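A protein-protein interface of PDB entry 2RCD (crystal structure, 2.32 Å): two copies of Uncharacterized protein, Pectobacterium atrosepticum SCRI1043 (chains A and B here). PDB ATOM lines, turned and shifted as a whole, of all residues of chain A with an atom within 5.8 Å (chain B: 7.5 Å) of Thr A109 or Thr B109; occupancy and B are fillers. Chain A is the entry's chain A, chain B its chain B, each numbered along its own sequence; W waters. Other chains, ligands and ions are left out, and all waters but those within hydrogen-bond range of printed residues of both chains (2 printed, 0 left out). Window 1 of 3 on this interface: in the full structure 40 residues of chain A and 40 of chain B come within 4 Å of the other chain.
Printed residues of chain B within 4 Å of Ala A89: Met B88. Printed residues of chain B within 4 Å of Val A90: Thr B109 (3.7 Å) and Ala B121 (3.6 Å). Thr A109 touches just these residues of chain B: Met B88 (3.8 Å), Val B90 (3.9 Å) and Thr B109 (2.7 Å). Of the printed residues of chain B, Ala A122 touches Met B107. Printed residues of chain A within 4 Å of Tyr B84: Val A120. Of chain A, only Val A90 and Thr A109 come within 4 Å of Thr B109. Arg B118 touches none of the printed residues of chain A. Printed residues of chain A within 4 Å of Ala B122: Met A107. The nearest residue of chain B that does not touch Thr A109 is Met B107 (5.5 Å). The nearest residue of chain A that does not touch Thr B109 is Met A107 (5.4 Å). The nearest printed residue of chain B that does not touch Ala A89 is Thr B109 (5.7 Å).
OG1 of Thr B109 lies within hydrogen-bond range of OG1 of Thr A109 (2.7 Å). The backbone NH (N) of Ala A122 is in hydrogen-bond range of the side-chain sulfur (SD) of Met B107, at 3.6 Å. The side-chain sulfur (SD) of Met A107 lies within hydrogen-bond range of the backbone NH (N) of Ala B122 (3.6 Å).
Hydrophobic or aromatic side chains of chain B within 4 Å of the printed part of chain A: Tyr B84, Met B88, Val B90, Met B107, Ala B121 and His B123. Printed residues of chain A that touch a printed residue of chain B: Ala A89, Val A90, Met A107, Thr A109, Val A120, Ala A121 and Ala A122. Hydrophobic or aromatic side chains of chain A within 4 Å of the printed part of chain B: Val A90, Met A107, Val A120 and Ala A121.
The backbone NH of Met B107 lies within hydrogen-bond range of the backbone carbonyl oxygen of His B123. The backbone NH (N) of Ala A89 lies within hydrogen-bond range of the backbone carbonyl oxygen (O) of Trp A110, 2.8 Å away. The backbone carbonyl oxygen of Thr A109 lies within hydrogen-bond range of the backbone NH of Val A120, at 3.0 Å. The backbone NH of Thr A109 is in hydrogen-bond range of the backbone carbonyl oxygen of Ala A121, at 2.9 Å. The backbone NH (N) of Thr B109 lies within hydrogen-bond range of the backbone carbonyl oxygen (O) of Ala B121, 3.0 Å away. N of Val B120 is in hydrogen-bond range of O of Thr B109, 2.9 Å away.
Val A90 touches Thr B109, and with the chains exchanged Thr A109 touches Val B90. Val A90 touches Ala B121, and with the chains exchanged Ala A121 touches Val B90. Met A107 touches Ala B122, and with the chains exchanged Ala A122 touches Met B107. Thr A109 touches its own counterpart, Thr B109. Positions printed for both chains: 89, 90, 91, 107, 108, 109, 110, 111, 118, 119, 120, 121 and 122. Of the 13 pairs that touch across the chains among the printed residues, 9 have their exchanged pair printed and touching as well.
Among the printed residues, pairs that only touch across the chains: Val A120 with Tyr B84 (3.2 Å), Ala A121 with Val B90 (3.5 Å), Ala A121 with Met B107 (3.6 Å), Met A107 with Ala B121 (3.6 Å), Val A90 with Ala B121 (3.6 Å), Val A90 with Thr B109 (3.7 Å), Met A107 with His B123 (3.7 Å), Thr A109 with Met B88 (3.8 Å), Ala A89 with Met B88 (3.9 Å) and Thr A109 with Val B90 (3.9 Å).
Water W1 bridges the side-chain hydroxyl of Thr B109 (2.7 Å) and the side-chain sulfur of Met A107 (3.4 Å). Water W2 lies within hydrogen-bond range of the side-chain hydroxyl of Thr A109 (3.0 Å) and the side-chain sulfur of Met B107 (3.3 Å).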
ATOM      1  N   ALA A  89      21.559  -3.351  23.335  1.00  0.00           N
ATOM      2  CA  ALA A  89      23.011  -3.519  23.223  1.00  0.00           C
ATOM      3  C   ALA A  89      23.405  -4.860  22.573  1.00  0.00           C
ATOM      4  O   ALA A  89      22.610  -5.846  22.574  1.00  0.00           O
ATOM      5  CB  ALA A  89      23.671  -3.377  24.591  1.00  0.00           C
ATOM      6  N   VAL A  90      24.592  -4.859  21.951  1.00  0.00           N
ATOM      7  CA  VAL A  90      25.179  -6.072  21.411  1.00  0.00           C
ATOM      8  C   VAL A  90      26.545  -6.246  22.019  1.00  0.00           C
ATOM      9  O   VAL A  90      27.370  -5.311  22.029  1.00  0.00           O
ATOM     10  CB  VAL A  90      25.214  -6.164  19.886  1.00  0.00           C
ATOM     11  CG1 VAL A  90      25.820  -7.499  19.487  1.00  0.00           C
ATOM     12  CG2 VAL A  90      23.801  -6.083  19.337  1.00  0.00           C
ATOM     13  N   ALA A  91      26.732  -7.396  22.668  1.00  0.00           N
ATOM     14  CA  ALA A  91      28.032  -7.753  23.257  1.00  0.00           C
ATOM     15  C   ALA A  91      28.540  -8.903  22.394  1.00  0.00           C
ATOM     16  O   ALA A  91      27.785  -9.864  22.107  1.00  0.00           O
ATOM     17  CB  ALA A  91      27.901  -8.164  24.707  1.00  0.00           C
ATOM     18  N   MET A 107      28.043 -14.140  20.968  1.00  0.00           N
ATOM     19  CA  MET A 107      27.330 -12.939  20.630  1.00  0.00           C
ATOM     20  C   MET A 107      26.021 -12.911  21.437  1.00  0.00           C
ATOM     21  O   MET A 107      25.335 -13.895  21.510  1.00  0.00           O
ATOM     22  CB  MET A 107      27.080 -12.895  19.129  1.00  0.00           C
ATOM     23  CG  MET A 107      26.592 -11.550  18.694  1.00  0.00           C
ATOM     24  SD  MET A 107      26.445 -11.411  16.781  1.00  0.00           S
ATOM     25  CE  MET A 107      28.311 -11.176  16.262  1.00  0.00           C
ATOM     26  N   GLN A 108      25.706 -11.768  22.033  1.00  0.00           N
ATOM     27  CA  GLN A 108      24.516 -11.604  22.854  1.00  0.00           C
ATOM     28  C   GLN A 108      23.869 -10.301  22.578  1.00  0.00           C
ATOM     29  O   GLN A 108      24.540  -9.266  22.557  1.00  0.00           O
ATOM     30  CB  GLN A 108      24.903 -11.515  24.340  1.00  0.00           C
ATOM     31  CG  GLN A 108      25.584 -12.718  24.900  1.00  0.00           C
ATOM     32  CD  GLN A 108      26.061 -12.484  26.321  1.00  0.00           C
ATOM     33  OE1 GLN A 108      26.459 -11.369  26.702  1.00  0.00           O
ATOM     34  NE2 GLN A 108      26.036 -13.552  27.115  1.00  0.00           N
ATOM     35  N   THR A 109      22.561 -10.329  22.433  1.00  0.00           N
ATOM     36  CA  THR A 109      21.803  -9.089  22.325  1.00  0.00           C
ATOM     37  C   THR A 109      21.050  -8.830  23.641  1.00  0.00           C
ATOM     38  O   THR A 109      20.260  -9.665  24.092  1.00  0.00           O
ATOM     39  CB  THR A 109      20.853  -9.123  21.167  1.00  0.00           C
ATOM     40  OG1 THR A 109      21.589  -9.492  19.991  1.00  0.00           O
ATOM     41  CG2 THR A 109      20.164  -7.740  20.987  1.00  0.00           C
ATOM     42  N   TRP A 110      21.382  -7.701  24.266  1.00  0.00           N
ATOM     43  CA  TRP A 110      20.792  -7.241  25.510  1.00  0.00           C
ATOM     44  C   TRP A 110      19.716  -6.180  25.291  1.00  0.00           C
ATOM     45  O   TRP A 110      19.886  -5.294  24.444  1.00  0.00           O
ATOM     46  CB  TRP A 110      21.872  -6.567  26.321  1.00  0.00           C
ATOM     47  CG  TRP A 110      22.929  -7.484  26.769  1.00  0.00           C
ATOM     48  CD1 TRP A 110      24.012  -7.907  26.072  1.00  0.00           C
ATOM     49  CD2 TRP A 110      23.016  -8.091  28.048  1.00  0.00           C
ATOM     50  NE1 TRP A 110      24.767  -8.764  26.831  1.00  0.00           N
ATOM     51  CE2 TRP A 110      24.177  -8.881  28.057  1.00  0.00           C
ATOM     52  CE3 TRP A 110      22.205  -8.063  29.188  1.00  0.00           C
ATOM     53  CZ2 TRP A 110      24.545  -9.625  29.154  1.00  0.00           C
ATOM     54  CZ3 TRP A 110      22.580  -8.789  30.276  1.00  0.00           C
ATOM     55  CH2 TRP A 110      23.731  -9.571  30.254  1.00  0.00           C
ATOM     56  N   VAL A 111      18.617  -6.266  26.044  1.00  0.00           N
ATOM     57  CA  VAL A 111      17.556  -5.247  26.045  1.00  0.00           C
ATOM     58  C   VAL A 111      17.208  -4.840  27.490  1.00  0.00           C
ATOM     59  O   VAL A 111      17.117  -5.685  28.365  1.00  0.00           O
ATOM     60  CB  VAL A 111      16.283  -5.693  25.291  1.00  0.00           C
ATOM     61  CG1 VAL A 111      15.312  -4.540  25.235  1.00  0.00           C
ATOM     62  CG2 VAL A 111      16.627  -6.134  23.858  1.00  0.00           C
ATOM     63  N   ARG A 118      18.605  -7.560  30.092  1.00  0.00           N
ATOM     64  CA  ARG A 118      18.347  -8.972  29.901  1.00  0.00           C
ATOM     65  C   ARG A 118      18.801  -9.415  28.546  1.00  0.00           C
ATOM     66  O   ARG A 118      18.599  -8.710  27.575  1.00  0.00           O
ATOM     67  CB  ARG A 118      16.839  -9.226  29.992  1.00  0.00           C
ATOM     68  CG  ARG A 118      16.212  -9.087  31.384  1.00  0.00           C
ATOM     69  CD  ARG A 118      16.595 -10.235  32.235  1.00  0.00           C
ATOM     70  NE  ARG A 118      16.026 -10.127  33.562  1.00  0.00           N
ATOM     71  CZ  ARG A 118      16.515  -9.390  34.561  1.00  0.00           C
ATOM     72  NH1 ARG A 118      17.588  -8.639  34.411  1.00  0.00           N
ATOM     73  NH2 ARG A 118      15.894  -9.393  35.734  1.00  0.00           N
ATOM     74  N   ILE A 119      19.375 -10.607  28.471  1.00  0.00           N
ATOM     75  CA  ILE A 119      19.830 -11.188  27.214  1.00  0.00           C
ATOM     76  C   ILE A 119      18.624 -11.844  26.568  1.00  0.00           C
ATOM     77  O   ILE A 119      18.119 -12.820  27.063  1.00  0.00           O
ATOM     78  CB  ILE A 119      20.957 -12.273  27.431  1.00  0.00           C
ATOM     79  CG1 ILE A 119      22.150 -11.697  28.209  1.00  0.00           C
ATOM     80  CG2 ILE A 119      21.474 -12.793  26.128  1.00  0.00           C
ATOM     81  CD1 ILE A 119      23.106 -12.732  28.742  1.00  0.00           C
ATOM     82  N   VAL A 120      18.191 -11.300  25.442  1.00  0.00           N
ATOM     83  CA  VAL A 120      17.076 -11.842  24.653  1.00  0.00           C
ATOM     84  C   VAL A 120      17.518 -12.880  23.618  1.00  0.00           C
ATOM     85  O   VAL A 120      16.696 -13.673  23.146  1.00  0.00           O
ATOM     86  CB  VAL A 120      16.307 -10.711  23.949  1.00  0.00           C
ATOM     87  CG1 VAL A 120      15.731  -9.732  24.984  1.00  0.00           C
ATOM     88  CG2 VAL A 120      17.227  -9.955  22.942  1.00  0.00           C
ATOM     89  N   ALA A 121      18.800 -12.893  23.248  1.00  0.00           N
ATOM     90  CA  ALA A 121      19.278 -13.903  22.263  1.00  0.00           C
ATOM     91  C   ALA A 121      20.753 -14.019  22.392  1.00  0.00           C
ATOM     92  O   ALA A 121      21.403 -13.006  22.681  1.00  0.00           O
ATOM     93  CB  ALA A 121      18.880 -13.557  20.773  1.00  0.00           C
ATOM     94  N   ALA A 122      21.280 -15.248  22.287  1.00  0.00           N
ATOM     95  CA  ALA A 122      22.744 -15.472  22.377  1.00  0.00           C
ATOM     96  C   ALA A 122      23.130 -16.613  21.475  1.00  0.00           C
ATOM     97  O   ALA A 122      22.379 -17.561  21.332  1.00  0.00           O
ATOM     98  CB  ALA A 122      23.250 -15.750  23.819  1.00  0.00           C
ATOM     99  N   LEU B  38      22.733  -4.257   3.216  1.00  0.00           N
ATOM    100  CA  LEU B  38      22.022  -4.680   4.420  1.00  0.00           C
ATOM    101  C   LEU B  38      22.837  -4.742   5.693  1.00  0.00           C
ATOM    102  O   LEU B  38      22.261  -4.802   6.757  1.00  0.00           O
ATOM    103  CB  LEU B  38      21.296  -6.016   4.187  1.00  0.00           C
ATOM    104  CG  LEU B  38      20.136  -5.879   3.205  1.00  0.00           C
ATOM    105  CD1 LEU B  38      19.578  -7.272   2.873  1.00  0.00           C
ATOM    106  CD2 LEU B  38      19.016  -4.911   3.730  1.00  0.00           C
ATOM    107  N   TRP B  40      25.393  -2.985   8.394  1.00  0.00           N
ATOM    108  CA  TRP B  40      25.682  -1.646   8.854  1.00  0.00           C
ATOM    109  C   TRP B  40      27.071  -1.306   8.434  1.00  0.00           C
ATOM    110  O   TRP B  40      27.995  -2.077   8.645  1.00  0.00           O
ATOM    111  CB  TRP B  40      25.568  -1.613  10.352  1.00  0.00           C
ATOM    112  CG  TRP B  40      25.780  -0.331  10.994  1.00  0.00           C
ATOM    113  CD1 TRP B  40      25.397   0.895  10.551  1.00  0.00           C
ATOM    114  CD2 TRP B  40      26.296  -0.151  12.295  1.00  0.00           C
ATOM    115  NE1 TRP B  40      25.730   1.854  11.480  1.00  0.00           N
ATOM    116  CE2 TRP B  40      26.273   1.235  12.568  1.00  0.00           C
ATOM    117  CE3 TRP B  40      26.832  -1.012  13.239  1.00  0.00           C
ATOM    118  CZ2 TRP B  40      26.738   1.767  13.759  1.00  0.00           C
ATOM    119  CZ3 TRP B  40      27.288  -0.478  14.430  1.00  0.00           C
ATOM    120  CH2 TRP B  40      27.243   0.898  14.675  1.00  0.00           C
ATOM    121  N   TYR B  84      11.754  -5.434  18.867  1.00  0.00           N
ATOM    122  CA  TYR B  84      11.750  -4.769  20.151  1.00  0.00           C
ATOM    123  C   TYR B  84      11.494  -3.289  19.879  1.00  0.00           C
ATOM    124  O   TYR B  84      12.313  -2.610  19.253  1.00  0.00           O
ATOM    125  CB  TYR B  84      13.089  -5.020  20.814  1.00  0.00           C
ATOM    126  CG  TYR B  84      13.305  -6.493  21.087  1.00  0.00           C
ATOM    127  CD1 TYR B  84      12.685  -7.091  22.163  1.00  0.00           C
ATOM    128  CD2 TYR B  84      14.118  -7.282  20.274  1.00  0.00           C
ATOM    129  CE1 TYR B  84      12.858  -8.406  22.434  1.00  0.00           C
ATOM    130  CE2 TYR B  84      14.283  -8.625  20.532  1.00  0.00           C
ATOM    131  CZ  TYR B  84      13.642  -9.165  21.630  1.00  0.00           C
ATOM    132  OH  TYR B  84      13.755 -10.478  21.978  1.00  0.00           O
ATOM    133  N   MET B  88      14.464  -2.279  16.578  1.00  0.00           N
ATOM    134  CA  MET B  88      15.473  -3.325  16.784  1.00  0.00           C
ATOM    135  C   MET B  88      14.806  -4.652  16.653  1.00  0.00           C
ATOM    136  O   MET B  88      13.639  -4.808  16.984  1.00  0.00           O
ATOM    137  CB  MET B  88      16.166  -3.282  18.130  1.00  0.00           C
ATOM    138  CG  MET B  88      17.522  -4.160  18.184  1.00  0.00           C
ATOM    139  SD  MET B  88      18.296  -4.622  19.976  1.00  0.00           S
ATOM    140  CE  MET B  88      20.250  -3.998  19.768  1.00  0.00           C
ATOM    141  N   ALA B  89      15.547  -5.616  16.152  1.00  0.00           N
ATOM    142  CA  ALA B  89      15.019  -6.945  15.967  1.00  0.00           C
ATOM    143  C   ALA B  89      16.152  -7.938  16.095  1.00  0.00           C
ATOM    144  O   ALA B  89      17.337  -7.575  16.042  1.00  0.00           O
ATOM    145  CB  ALA B  89      14.330  -7.047  14.592  1.00  0.00           C
ATOM    146  N   VAL B  90      15.787  -9.177  16.368  1.00  0.00           N
ATOM    147  CA  VAL B  90      16.744 -10.259  16.392  1.00  0.00           C
ATOM    148  C   VAL B  90      16.124 -11.332  15.536  1.00  0.00           C
ATOM    149  O   VAL B  90      14.974 -11.660  15.757  1.00  0.00           O
ATOM    150  CB  VAL B  90      17.062 -10.792  17.806  1.00  0.00           C
ATOM    151  CG1 VAL B  90      17.900 -12.097  17.713  1.00  0.00           C
ATOM    152  CG2 VAL B  90      17.807  -9.720  18.649  1.00  0.00           C
ATOM    153  N   ALA B  91      16.851 -11.805  14.518  1.00  0.00           N
ATOM    154  CA  ALA B  91      16.385 -12.912  13.656  1.00  0.00           C
ATOM    155  C   ALA B  91      17.290 -14.126  13.905  1.00  0.00           C
ATOM    156  O   ALA B  91      18.523 -13.996  13.870  1.00  0.00           O
ATOM    157  CB  ALA B  91      16.423 -12.501  12.233  1.00  0.00           C
ATOM    158  N   SER B  92      16.719 -15.278  14.234  1.00  0.00           N
ATOM    159  CA  SER B  92      17.538 -16.464  14.508  1.00  0.00           C
ATOM    160  C   SER B  92      16.945 -17.557  13.725  1.00  0.00           C
ATOM    161  O   SER B  92      15.730 -17.626  13.635  1.00  0.00           O
ATOM    162  CB  SER B  92      17.489 -16.895  15.969  1.00  0.00           C
ATOM    163  OG  SER B  92      17.787 -15.821  16.810  1.00  0.00           O
ATOM    164  N   MET B 107      22.312 -16.082  13.641  1.00  0.00           N
ATOM    165  CA  MET B 107      21.656 -15.103  14.490  1.00  0.00           C
ATOM    166  C   MET B 107      22.048 -13.702  14.029  1.00  0.00           C
ATOM    167  O   MET B 107      23.219 -13.411  13.893  1.00  0.00           O
ATOM    168  CB  MET B 107      22.037 -15.294  15.940  1.00  0.00           C
ATOM    169  CG  MET B 107      21.335 -14.321  16.908  1.00  0.00           C
ATOM    170  SD  MET B 107      21.639 -14.822  18.759  1.00  0.00           S
ATOM    171  CE  MET B 107      20.258 -16.258  18.830  1.00  0.00           C
ATOM    172  N   GLN B 108      21.062 -12.832  13.834  1.00  0.00           N
ATOM    173  CA  GLN B 108      21.295 -11.449  13.363  1.00  0.00           C
ATOM    174  C   GLN B 108      20.595 -10.456  14.231  1.00  0.00           C
ATOM    175  O   GLN B 108      19.461 -10.639  14.575  1.00  0.00           O
ATOM    176  CB  GLN B 108      20.679 -11.293  11.962  1.00  0.00           C
ATOM    177  CG  GLN B 108      21.270 -12.192  10.922  1.00  0.00           C
ATOM    178  CD  GLN B 108      20.575 -12.097   9.581  1.00  0.00           C
ATOM    179  OE1 GLN B 108      19.356 -11.899   9.499  1.00  0.00           O
ATOM    180  NE2 GLN B 108      21.348 -12.296   8.510  1.00  0.00           N
ATOM    181  N   THR B 109      21.254  -9.375  14.552  1.00  0.00           N
ATOM    182  CA  THR B 109      20.630  -8.263  15.291  1.00  0.00           C
ATOM    183  C   THR B 109      20.448  -7.106  14.302  1.00  0.00           C
ATOM    184  O   THR B 109      21.420  -6.621  13.745  1.00  0.00           O
ATOM    185  CB  THR B 109      21.481  -7.842  16.461  1.00  0.00           C
ATOM    186  OG1 THR B 109      21.684  -8.980  17.313  1.00  0.00           O
ATOM    187  CG2 THR B 109      20.806  -6.696  17.257  1.00  0.00           C
ATOM    188  N   TRP B 110      19.194  -6.724  14.066  1.00  0.00           N
ATOM    189  CA  TRP B 110      18.821  -5.656  13.134  1.00  0.00           C
ATOM    190  C   TRP B 110      18.383  -4.352  13.819  1.00  0.00           C
ATOM    191  O   TRP B 110      17.623  -4.388  14.776  1.00  0.00           O
ATOM    192  CB  TRP B 110      17.654  -6.107  12.274  1.00  0.00           C
ATOM    193  CG  TRP B 110      17.898  -7.248  11.338  1.00  0.00           C
ATOM    194  CD1 TRP B 110      17.909  -8.593  11.637  1.00  0.00           C
ATOM    195  CD2 TRP B 110      18.035  -7.159   9.922  1.00  0.00           C
ATOM    196  NE1 TRP B 110      18.078  -9.348  10.489  1.00  0.00           N
ATOM    197  CE2 TRP B 110      18.164  -8.496   9.421  1.00  0.00           C
ATOM    198  CE3 TRP B 110      18.072  -6.089   9.020  1.00  0.00           C
ATOM    199  CZ2 TRP B 110      18.334  -8.771   8.063  1.00  0.00           C
ATOM    200  CZ3 TRP B 110      18.247  -6.366   7.659  1.00  0.00           C
ATOM    201  CH2 TRP B 110      18.370  -7.698   7.197  1.00  0.00           C
ATOM    202  N   VAL B 111      18.883  -3.222  13.323  1.00  0.00           N
ATOM    203  CA  VAL B 111      18.522  -1.880  13.789  1.00  0.00           C
ATOM    204  C   VAL B 111      17.971  -1.031  12.591  1.00  0.00           C
ATOM    205  O   VAL B 111      18.492  -1.080  11.484  1.00  0.00           O
ATOM    206  CB  VAL B 111      19.716  -1.227  14.490  1.00  0.00           C
ATOM    207  CG1 VAL B 111      19.368   0.133  15.033  1.00  0.00           C
ATOM    208  CG2 VAL B 111      20.186  -2.113  15.660  1.00  0.00           C
ATOM    209  N   MET B 113      17.863   2.055  10.661  1.00  0.00           N
ATOM    210  CA  MET B 113      18.629   3.257  10.445  1.00  0.00           C
ATOM    211  C   MET B 113      17.785   4.125   9.491  1.00  0.00           C
ATOM    212  O   MET B 113      16.799   3.647   8.915  1.00  0.00           O
ATOM    213  CB  MET B 113      19.939   2.892   9.739  1.00  0.00           C
ATOM    214  CG  MET B 113      20.743   1.758  10.348  1.00  0.00           C
ATOM    215  SD  MET B 113      21.888   2.292  11.773  1.00  0.00           S
ATOM    216  CE  MET B 113      22.325   0.546  12.543  1.00  0.00           C
ATOM    217  N   TRP B 117      16.537  -0.808   7.562  1.00  0.00           N
ATOM    218  CA  TRP B 117      16.884  -1.908   8.450  1.00  0.00           C
ATOM    219  C   TRP B 117      18.269  -2.389   8.117  1.00  0.00           C
ATOM    220  O   TRP B 117      18.589  -2.594   6.966  1.00  0.00           O
ATOM    221  CB  TRP B 117      15.879  -3.055   8.332  1.00  0.00           C
ATOM    222  CG  TRP B 117      14.587  -2.751   9.025  1.00  0.00           C
ATOM    223  CD1 TRP B 117      13.422  -2.334   8.451  1.00  0.00           C
ATOM    224  CD2 TRP B 117      14.353  -2.777  10.439  1.00  0.00           C
ATOM    225  NE1 TRP B 117      12.460  -2.129   9.423  1.00  0.00           N
ATOM    226  CE2 TRP B 117      13.007  -2.392  10.650  1.00  0.00           C
ATOM    227  CE3 TRP B 117      15.150  -3.087  11.550  1.00  0.00           C
ATOM    228  CZ2 TRP B 117      12.439  -2.317  11.923  1.00  0.00           C
ATOM    229  CZ3 TRP B 117      14.572  -3.031  12.826  1.00  0.00           C
ATOM    230  CH2 TRP B 117      13.239  -2.648  12.995  1.00  0.00           C
ATOM    231  N   ARG B 118      19.101  -2.539   9.137  1.00  0.00           N
ATOM    232  CA  ARG B 118      20.483  -2.958   8.953  1.00  0.00           C
ATOM    233  C   ARG B 118      20.954  -3.935  10.014  1.00  0.00           C
ATOM    234  O   ARG B 118      20.685  -3.740  11.197  1.00  0.00           O
ATOM    235  CB  ARG B 118      21.367  -1.735   9.016  1.00  0.00           C
ATOM    236  CG  ARG B 118      21.182  -0.736   7.852  1.00  0.00           C
ATOM    237  CD  ARG B 118      21.848  -1.228   6.610  1.00  0.00           C
ATOM    238  NE  ARG B 118      21.804  -0.222   5.544  1.00  0.00           N
ATOM    239  CZ  ARG B 118      20.787  -0.047   4.702  1.00  0.00           C
ATOM    240  NH1 ARG B 118      19.688  -0.771   4.781  1.00  0.00           N
ATOM    241  NH2 ARG B 118      20.878   0.861   3.754  1.00  0.00           N
ATOM    242  N   ILE B 119      21.658  -4.978   9.573  1.00  0.00           N
ATOM    243  CA  ILE B 119      22.272  -5.960  10.458  1.00  0.00           C
ATOM    244  C   ILE B 119      23.508  -5.284  11.057  1.00  0.00           C
ATOM    245  O   ILE B 119      24.413  -4.945  10.325  1.00  0.00           O
ATOM    246  CB  ILE B 119      22.768  -7.199   9.667  1.00  0.00           C
ATOM    247  CG1 ILE B 119      21.610  -7.916   8.973  1.00  0.00           C
ATOM    248  CG2 ILE B 119      23.510  -8.195  10.570  1.00  0.00           C
ATOM    249  CD1 ILE B 119      22.092  -8.802   7.878  1.00  0.00           C
ATOM    250  N   VAL B 120      23.515  -5.083  12.377  1.00  0.00           N
ATOM    251  CA  VAL B 120      24.662  -4.514  13.109  1.00  0.00           C
ATOM    252  C   VAL B 120      25.625  -5.578  13.700  1.00  0.00           C
ATOM    253  O   VAL B 120      26.762  -5.261  14.005  1.00  0.00           O
ATOM    254  CB  VAL B 120      24.173  -3.552  14.237  1.00  0.00           C
ATOM    255  CG1 VAL B 120      23.282  -2.445  13.626  1.00  0.00           C
ATOM    256  CG2 VAL B 120      23.416  -4.309  15.321  1.00  0.00           C
ATOM    257  N   ALA B 121      25.154  -6.815  13.856  1.00  0.00           N
ATOM    258  CA  ALA B 121      25.974  -7.942  14.362  1.00  0.00           C
ATOM    259  C   ALA B 121      25.357  -9.273  13.927  1.00  0.00           C
ATOM    260  O   ALA B 121      24.165  -9.422  14.045  1.00  0.00           O
ATOM    261  CB  ALA B 121      26.066  -7.909  15.869  1.00  0.00           C
ATOM    262  N   ALA B 122      26.176 -10.207  13.430  1.00  0.00           N
ATOM    263  CA  ALA B 122      25.717 -11.496  12.957  1.00  0.00           C
ATOM    264  C   ALA B 122      26.682 -12.591  13.376  1.00  0.00           C
ATOM    265  O   ALA B 122      27.882 -12.384  13.438  1.00  0.00           O
ATOM    266  CB  ALA B 122      25.541 -11.501  11.443  1.00  0.00           C
ATOM    267  N   HIS B 123      26.141 -13.746  13.727  1.00  0.00           N
ATOM    268  CA  HIS B 123      26.946 -14.890  14.144  1.00  0.00           C
ATOM    269  C   HIS B 123      26.361 -16.096  13.426  1.00  0.00           C
ATOM    270  O   HIS B 123      25.153 -16.352  13.536  1.00  0.00           O
ATOM    271  CB  HIS B 123      26.843 -15.071  15.651  1.00  0.00           C
ATOM    272  CG  HIS B 123      27.765 -16.099  16.242  1.00  0.00           C
ATOM    273  ND1 HIS B 123      28.040 -16.132  17.591  1.00  0.00           N
ATOM    274  CD2 HIS B 123      28.457 -17.126  15.692  1.00  0.00           C
ATOM    275  CE1 HIS B 123      28.844 -17.150  17.848  1.00  0.00           C
ATOM    276  NE2 HIS B 123      29.112 -17.767  16.712  1.00  0.00           N
HETATM  277  O   HOH W   1      23.021 -11.251  16.873  1.00  0.00           O
HETATM  278  O   HOH W   2      23.130 -11.970  19.527  1.00  0.00           O
